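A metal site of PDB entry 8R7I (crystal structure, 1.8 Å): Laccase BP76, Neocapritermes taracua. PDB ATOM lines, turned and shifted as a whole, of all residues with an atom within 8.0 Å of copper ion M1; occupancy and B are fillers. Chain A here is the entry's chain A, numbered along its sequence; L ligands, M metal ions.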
ATOM      1  N   HIS A 116     -32.794  30.320  -2.295  1.00  0.00           N
ATOM      2  CA  HIS A 116     -33.287  29.706  -3.537  1.00  0.00           C
ATOM      3  C   HIS A 116     -33.009  28.185  -3.492  1.00  0.00           C
ATOM      4  O   HIS A 116     -31.914  27.738  -3.044  1.00  0.00           O
ATOM      5  CB  HIS A 116     -32.614  30.380  -4.743  1.00  0.00           C
ATOM      6  CG  HIS A 116     -32.839  29.635  -6.000  1.00  0.00           C
ATOM      7  ND1 HIS A 116     -34.115  29.428  -6.510  1.00  0.00           N
ATOM      8  CD2 HIS A 116     -31.967  29.077  -6.884  1.00  0.00           C
ATOM      9  CE1 HIS A 116     -34.008  28.767  -7.655  1.00  0.00           C
ATOM     10  NE2 HIS A 116     -32.745  28.565  -7.884  1.00  0.00           N
ATOM     11  N   TRP A 117     -34.021  27.385  -3.920  1.00  0.00           N
ATOM     12  CA  TRP A 117     -33.951  25.928  -3.927  1.00  0.00           C
ATOM     13  C   TRP A 117     -33.597  25.542  -5.363  1.00  0.00           C
ATOM     14  O   TRP A 117     -34.482  25.333  -6.194  1.00  0.00           O
ATOM     15  CB  TRP A 117     -35.257  25.349  -3.378  1.00  0.00           C
ATOM     16  CG  TRP A 117     -35.728  26.182  -2.215  1.00  0.00           C
ATOM     17  CD1 TRP A 117     -36.595  27.226  -2.305  1.00  0.00           C
ATOM     18  CD2 TRP A 117     -35.258  26.164  -0.854  1.00  0.00           C
ATOM     19  NE1 TRP A 117     -36.745  27.842  -1.076  1.00  0.00           N
ATOM     20  CE2 TRP A 117     -35.907  27.231  -0.180  1.00  0.00           C
ATOM     21  CE3 TRP A 117     -34.376  25.368  -0.145  1.00  0.00           C
ATOM     22  CZ2 TRP A 117     -35.687  27.513   1.174  1.00  0.00           C
ATOM     23  CZ3 TRP A 117     -34.158  25.630   1.209  1.00  0.00           C
ATOM     24  CH2 TRP A 117     -34.806  26.707   1.837  1.00  0.00           C
ATOM     25  N   HIS A 118     -32.302  25.578  -5.649  1.00  0.00           N
ATOM     26  CA  HIS A 118     -31.744  25.450  -7.001  1.00  0.00           C
ATOM     27  C   HIS A 118     -32.022  24.034  -7.549  1.00  0.00           C
ATOM     28  O   HIS A 118     -31.544  23.032  -7.004  1.00  0.00           O
ATOM     29  CB  HIS A 118     -30.256  25.805  -6.939  1.00  0.00           C
ATOM     30  CG  HIS A 118     -29.529  25.668  -8.240  1.00  0.00           C
ATOM     31  ND1 HIS A 118     -28.662  26.638  -8.655  1.00  0.00           N
ATOM     32  CD2 HIS A 118     -29.417  24.672  -9.140  1.00  0.00           C
ATOM     33  CE1 HIS A 118     -28.095  26.257  -9.838  1.00  0.00           C
ATOM     34  NE2 HIS A 118     -28.543  25.081 -10.146  1.00  0.00           N
ATOM     35  N   GLY A 119     -32.769  23.982  -8.660  1.00  0.00           N
ATOM     36  CA  GLY A 119     -33.105  22.754  -9.370  1.00  0.00           C
ATOM     37  C   GLY A 119     -34.497  22.266  -9.019  1.00  0.00           C
ATOM     38  O   GLY A 119     -34.990  21.368  -9.712  1.00  0.00           O
ATOM     39  N   TYR A 158     -29.995  21.631  -4.785  1.00  0.00           N
ATOM     40  CA  TYR A 158     -29.020  22.525  -4.179  1.00  0.00           C
ATOM     41  C   TYR A 158     -29.774  23.705  -3.538  1.00  0.00           C
ATOM     42  O   TYR A 158     -30.824  24.067  -4.035  1.00  0.00           O
ATOM     43  CB  TYR A 158     -28.039  22.912  -5.305  1.00  0.00           C
ATOM     44  CG  TYR A 158     -26.917  23.872  -5.010  1.00  0.00           C
ATOM     45  CD1 TYR A 158     -26.151  23.781  -3.873  1.00  0.00           C
ATOM     46  CD2 TYR A 158     -26.543  24.839  -5.955  1.00  0.00           C
ATOM     47  CE1 TYR A 158     -25.086  24.626  -3.646  1.00  0.00           C
ATOM     48  CE2 TYR A 158     -25.487  25.686  -5.746  1.00  0.00           C
ATOM     49  CZ  TYR A 158     -24.757  25.599  -4.569  1.00  0.00           C
ATOM     50  OH  TYR A 158     -23.699  26.465  -4.338  1.00  0.00           O
ATOM     51  N   TRP A 159     -29.250  24.286  -2.456  1.00  0.00           N
ATOM     52  CA  TRP A 159     -29.846  25.498  -1.889  1.00  0.00           C
ATOM     53  C   TRP A 159     -28.746  26.510  -1.559  1.00  0.00           C
ATOM     54  O   TRP A 159     -27.598  26.117  -1.199  1.00  0.00           O
ATOM     55  CB  TRP A 159     -30.790  25.207  -0.709  1.00  0.00           C
ATOM     56  CG  TRP A 159     -30.141  24.687   0.538  1.00  0.00           C
ATOM     57  CD1 TRP A 159     -30.096  23.382   0.951  1.00  0.00           C
ATOM     58  CD2 TRP A 159     -29.422  25.437   1.547  1.00  0.00           C
ATOM     59  NE1 TRP A 159     -29.373  23.266   2.120  1.00  0.00           N
ATOM     60  CE2 TRP A 159     -28.969  24.507   2.508  1.00  0.00           C
ATOM     61  CE3 TRP A 159     -29.127  26.802   1.729  1.00  0.00           C
ATOM     62  CZ2 TRP A 159     -28.269  24.906   3.650  1.00  0.00           C
ATOM     63  CZ3 TRP A 159     -28.368  27.195   2.831  1.00  0.00           C
ATOM     64  CH2 TRP A 159     -27.962  26.240   3.769  1.00  0.00           C
ATOM     65  N   HIS A 160     -29.084  27.806  -1.721  1.00  0.00           N
ATOM     66  CA  HIS A 160     -28.137  28.866  -1.348  1.00  0.00           C
ATOM     67  C   HIS A 160     -28.864  30.175  -1.190  1.00  0.00           C
ATOM     68  O   HIS A 160     -29.937  30.368  -1.785  1.00  0.00           O
ATOM     69  CB  HIS A 160     -26.982  28.961  -2.374  1.00  0.00           C
ATOM     70  CG  HIS A 160     -27.469  29.182  -3.771  1.00  0.00           C
ATOM     71  ND1 HIS A 160     -27.700  30.428  -4.277  1.00  0.00           N
ATOM     72  CD2 HIS A 160     -27.720  28.319  -4.778  1.00  0.00           C
ATOM     73  CE1 HIS A 160     -28.095  30.326  -5.571  1.00  0.00           C
ATOM     74  NE2 HIS A 160     -28.056  29.035  -5.886  1.00  0.00           N
ATOM     75  N   SER A 161     -28.241  31.118  -0.468  1.00  0.00           N
ATOM     76  CA  SER A 161     -28.712  32.489  -0.462  1.00  0.00           C
ATOM     77  C   SER A 161     -28.722  32.989  -1.906  1.00  0.00           C
ATOM     78  O   SER A 161     -27.730  32.759  -2.639  1.00  0.00           O
ATOM     79  CB  SER A 161     -27.874  33.398   0.388  1.00  0.00           C
ATOM     80  OG  SER A 161     -28.280  34.723   0.148  1.00  0.00           O
ATOM     81  N   HIS A 162     -29.814  33.637  -2.300  1.00  0.00           N
ATOM     82  CA  HIS A 162     -29.921  34.328  -3.596  1.00  0.00           C
ATOM     83  C   HIS A 162     -29.910  35.846  -3.369  1.00  0.00           C
ATOM     84  O   HIS A 162     -30.439  36.603  -4.216  1.00  0.00           O
ATOM     85  CB  HIS A 162     -31.183  33.819  -4.331  1.00  0.00           C
ATOM     86  CG  HIS A 162     -30.984  33.772  -5.817  1.00  0.00           C
ATOM     87  ND1 HIS A 162     -30.810  34.943  -6.555  1.00  0.00           N
ATOM     88  CD2 HIS A 162     -30.877  32.737  -6.695  1.00  0.00           C
ATOM     89  CE1 HIS A 162     -30.656  34.599  -7.837  1.00  0.00           C
ATOM     90  NE2 HIS A 162     -30.711  33.267  -7.921  1.00  0.00           N
ATOM     91  N   LDO A 167     -23.740  33.650  -0.382  1.00  0.00           N
ATOM     92  CA  LDO A 167     -23.425  32.257  -0.658  1.00  0.00           C
ATOM     93  CB  LDO A 167     -23.740  31.845  -2.108  1.00  0.00           C
ATOM     94  CG  LDO A 167     -23.351  30.424  -2.454  1.00  0.00           C
ATOM     95  CD  LDO A 167     -23.452  30.139  -3.955  1.00  0.00           C
ATOM     96  CE  LDO A 167     -22.262  30.833  -4.652  1.00  0.00           C
ATOM     97  OZ  LDO A 167     -22.435  30.526  -6.064  1.00  0.00           O
ATOM     98  C   LDO A 167     -21.967  31.970  -0.330  1.00  0.00           C
ATOM     99  O   LDO A 167     -21.680  30.919   0.271  1.00  0.00           O
ATOM    100  N   GLY A 267     -21.424  21.370  -7.346  1.00  0.00           N
ATOM    101  CA  GLY A 267     -20.589  22.515  -7.681  1.00  0.00           C
ATOM    102  C   GLY A 267     -20.972  23.692  -6.784  1.00  0.00           C
ATOM    103  O   GLY A 267     -21.656  24.636  -7.234  1.00  0.00           O
ATOM    104  N   SER A 306     -19.804  26.092 -10.882  1.00  0.00           N
ATOM    105  CA  SER A 306     -20.842  26.759 -10.112  1.00  0.00           C
ATOM    106  C   SER A 306     -22.247  26.345 -10.539  1.00  0.00           C
ATOM    107  O   SER A 306     -22.660  26.658 -11.667  1.00  0.00           O
ATOM    108  CB  SER A 306     -20.659  28.289 -10.222  1.00  0.00           C
ATOM    109  OG  SER A 306     -21.547  28.949  -9.325  1.00  0.00           O
ATOM    110  N   GLY A 307     -22.987  25.671  -9.657  1.00  0.00           N
ATOM    111  CA  GLY A 307     -24.407  25.358  -9.816  1.00  0.00           C
ATOM    112  C   GLY A 307     -24.669  23.961 -10.426  1.00  0.00           C
ATOM    113  O   GLY A 307     -25.800  23.474 -10.345  1.00  0.00           O
ATOM    114  N   GLU A 308     -23.675  23.349 -11.094  1.00  0.00           N
ATOM    115  CA  GLU A 308     -23.846  22.011 -11.645  1.00  0.00           C
ATOM    116  C   GLU A 308     -23.823  20.948 -10.551  1.00  0.00           C
ATOM    117  O   GLU A 308     -23.185  21.144  -9.491  1.00  0.00           O
ATOM    118  CB  GLU A 308     -22.745  21.670 -12.659  1.00  0.00           C
ATOM    119  CG  GLU A 308     -22.703  22.576 -13.882  1.00  0.00           C
ATOM    120  CD  GLU A 308     -21.760  21.990 -14.912  1.00  0.00           C
ATOM    121  OE1 GLU A 308     -20.547  22.084 -14.667  1.00  0.00           O
ATOM    122  OE2 GLU A 308     -22.248  21.334 -15.882  1.00  0.00           O
ATOM    123  N   ARG A 309     -24.445  19.791 -10.831  1.00  0.00           N
ATOM    124  CA  ARG A 309     -24.318  18.576 -10.018  1.00  0.00           C
ATOM    125  C   ARG A 309     -24.065  17.394 -10.952  1.00  0.00           C
ATOM    126  O   ARG A 309     -24.723  17.301 -11.985  1.00  0.00           O
ATOM    127  CB  ARG A 309     -25.528  18.337  -9.096  1.00  0.00           C
ATOM    128  CG  ARG A 309     -25.752  19.394  -8.005  1.00  0.00           C
ATOM    129  CD  ARG A 309     -26.512  20.619  -8.492  1.00  0.00           C
ATOM    130  NE  ARG A 309     -27.849  20.248  -8.905  1.00  0.00           N
ATOM    131  CZ  ARG A 309     -28.593  20.839  -9.835  1.00  0.00           C
ATOM    132  NH1 ARG A 309     -28.134  21.876 -10.528  1.00  0.00           N
ATOM    133  NH2 ARG A 309     -29.810  20.393 -10.076  1.00  0.00           N
ATOM    134  N   HIS A 524     -27.759  29.262 -15.878  1.00  0.00           N
ATOM    135  CA  HIS A 524     -28.698  28.499 -15.083  1.00  0.00           C
ATOM    136  C   HIS A 524     -30.076  29.108 -15.275  1.00  0.00           C
ATOM    137  O   HIS A 524     -30.215  30.321 -15.171  1.00  0.00           O
ATOM    138  CB  HIS A 524     -28.251  28.493 -13.610  1.00  0.00           C
ATOM    139  CG  HIS A 524     -29.336  28.038 -12.705  1.00  0.00           C
ATOM    140  ND1 HIS A 524     -29.878  26.771 -12.795  1.00  0.00           N
ATOM    141  CD2 HIS A 524     -29.931  28.635 -11.651  1.00  0.00           C
ATOM    142  CE1 HIS A 524     -30.801  26.640 -11.860  1.00  0.00           C
ATOM    143  NE2 HIS A 524     -30.802  27.755 -11.173  1.00  0.00           N
ATOM    144  N   HIS A 526     -33.910  29.021 -13.763  1.00  0.00           N
ATOM    145  CA  HIS A 526     -34.862  28.681 -12.704  1.00  0.00           C
ATOM    146  C   HIS A 526     -36.132  28.052 -13.286  1.00  0.00           C
ATOM    147  O   HIS A 526     -36.505  28.360 -14.422  1.00  0.00           O
ATOM    148  CB  HIS A 526     -35.254  29.899 -11.879  1.00  0.00           C
ATOM    149  CG  HIS A 526     -34.180  30.510 -11.026  1.00  0.00           C
ATOM    150  ND1 HIS A 526     -34.475  31.001  -9.745  1.00  0.00           N
ATOM    151  CD2 HIS A 526     -32.873  30.776 -11.249  1.00  0.00           C
ATOM    152  CE1 HIS A 526     -33.336  31.464  -9.210  1.00  0.00           C
ATOM    153  NE2 HIS A 526     -32.368  31.349 -10.158  1.00  0.00           N
ATOM    154  N   ASP A 566     -29.819  21.825 -15.753  1.00  0.00           N
ATOM    155  CA  ASP A 566     -30.342  23.140 -15.427  1.00  0.00           C
ATOM    156  C   ASP A 566     -29.253  24.215 -15.409  1.00  0.00           C
ATOM    157  O   ASP A 566     -29.581  25.389 -15.295  1.00  0.00           O
ATOM    158  CB  ASP A 566     -31.224  23.134 -14.160  1.00  0.00           C
ATOM    159  CG  ASP A 566     -30.490  22.765 -12.889  1.00  0.00           C
ATOM    160  OD1 ASP A 566     -29.338  23.268 -12.680  1.00  0.00           O
ATOM    161  OD2 ASP A 566     -31.093  21.985 -12.090  1.00  0.00           O
ATOM    162  N   THR A 567     -27.977  23.820 -15.544  1.00  0.00           N
ATOM    163  CA  THR A 567     -26.844  24.729 -15.513  1.00  0.00           C
ATOM    164  C   THR A 567     -25.841  24.238 -16.578  1.00  0.00           C
ATOM    165  O   THR A 567     -25.463  23.088 -16.504  1.00  0.00           O
ATOM    166  CB  THR A 567     -26.205  24.782 -14.118  1.00  0.00           C
ATOM    167  OG1 THR A 567     -27.224  25.115 -13.165  1.00  0.00           O
ATOM    168  CG2 THR A 567     -25.085  25.783 -14.019  1.00  0.00           C
ATOM    169  N   HIS A 591     -29.422  33.182 -15.686  1.00  0.00           N
ATOM    170  CA  HIS A 591     -28.256  34.025 -15.364  1.00  0.00           C
ATOM    171  C   HIS A 591     -26.982  33.197 -15.268  1.00  0.00           C
ATOM    172  O   HIS A 591     -27.026  31.953 -15.074  1.00  0.00           O
ATOM    173  CB  HIS A 591     -28.518  34.805 -14.082  1.00  0.00           C
ATOM    174  CG  HIS A 591     -28.641  33.938 -12.896  1.00  0.00           C
ATOM    175  ND1 HIS A 591     -27.515  33.467 -12.220  1.00  0.00           N
ATOM    176  CD2 HIS A 591     -29.727  33.444 -12.237  1.00  0.00           C
ATOM    177  CE1 HIS A 591     -27.934  32.715 -11.185  1.00  0.00           C
ATOM    178  NE2 HIS A 591     -29.255  32.733 -11.172  1.00  0.00           N
ATOM    179  N   HIS A 593     -24.124  31.670 -13.340  1.00  0.00           N
ATOM    180  CA  HIS A 593     -24.122  31.221 -11.945  1.00  0.00           C
ATOM    181  C   HIS A 593     -22.869  31.721 -11.207  1.00  0.00           C
ATOM    182  O   HIS A 593     -22.846  31.684  -9.954  1.00  0.00           O
ATOM    183  CB  HIS A 593     -24.283  29.679 -11.857  1.00  0.00           C
ATOM    184  CG  HIS A 593     -24.951  29.307 -10.548  1.00  0.00           C
ATOM    185  ND1 HIS A 593     -24.211  29.058  -9.406  1.00  0.00           N
ATOM    186  CD2 HIS A 593     -26.251  29.190 -10.208  1.00  0.00           C
ATOM    187  CE1 HIS A 593     -25.033  28.795  -8.417  1.00  0.00           C
ATOM    188  NE2 HIS A 593     -26.293  28.818  -8.877  1.00  0.00           N
ATOM    189  N   LEU A 598     -23.512  37.442 -11.855  1.00  0.00           N
ATOM    190  CA  LEU A 598     -24.897  37.737 -11.485  1.00  0.00           C
ATOM    191  C   LEU A 598     -24.949  39.109 -10.802  1.00  0.00           C
ATOM    192  O   LEU A 598     -25.830  39.924 -11.099  1.00  0.00           O
ATOM    193  CB  LEU A 598     -25.451  36.639 -10.582  1.00  0.00           C
ATOM    194  CG  LEU A 598     -26.796  36.929  -9.943  1.00  0.00           C
ATOM    195  CD1 LEU A 598     -27.874  37.055 -10.995  1.00  0.00           C
ATOM    196  CD2 LEU A 598     -27.162  35.839  -8.931  1.00  0.00           C
HETATM  197  O1  LIG L   1     -29.201  30.433  -8.743  1.00  0.00           O
HETATM  198 CU    CU M   1     -28.096  28.363  -7.816  1.00  0.00          CU
HETATM  199 CU    CU M   2     -31.824  28.065  -9.554  1.00  0.00          CU
HETATM  200 CU    CU M   3     -30.494  32.102  -9.670  1.00  0.00          CU
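A ring nitrogen (NE2) of His 118 is in hydrogen-bond range of the guanidinium group of Arg 309 (3.3 Å).
ND1 of His 593 lies within hydrogen-bond range of OG of Ser 306 (2.7 Å).
The side-chain carboxylate of Asp 566 is in hydrogen-bond range of a ring nitrogen (NE2) of His 118, at 3.2 Å.
The side-chain hydroxyl (OG1) of Thr 567 is in hydrogen-bond range of a ring nitrogen (NE2) of His 118.
A ring nitrogen (NE2) of His 118 sits at hydrogen-bond distance from the backbone carbonyl oxygen (O) of Gly 307, at 3.2 Å.
O of His 160 is in hydrogen-bond range of N of His 116 (2.9 Å).
A ring nitrogen (NE2) of His 118 lies close to a ring nitrogen (ND1) of His 524 (3.4 Å).
The backbone carbonyl oxygen of Tyr 158 is in hydrogen-bond range of the backbone NH of His 118 (2.7 Å).
Of the 22 residues printed, 3 come within 4 Å of copper ion M1.
The nearest printed residue that does not touch copper ion M1 is His 116 (4.05 Å).
Copper ion M1 is bound by a ring nitrogen (ND1) of His 118, a ring nitrogen (NE2) of His 160, a ring nitrogen (NE2) of His 593 and an oxygen (O1) of the ligand.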
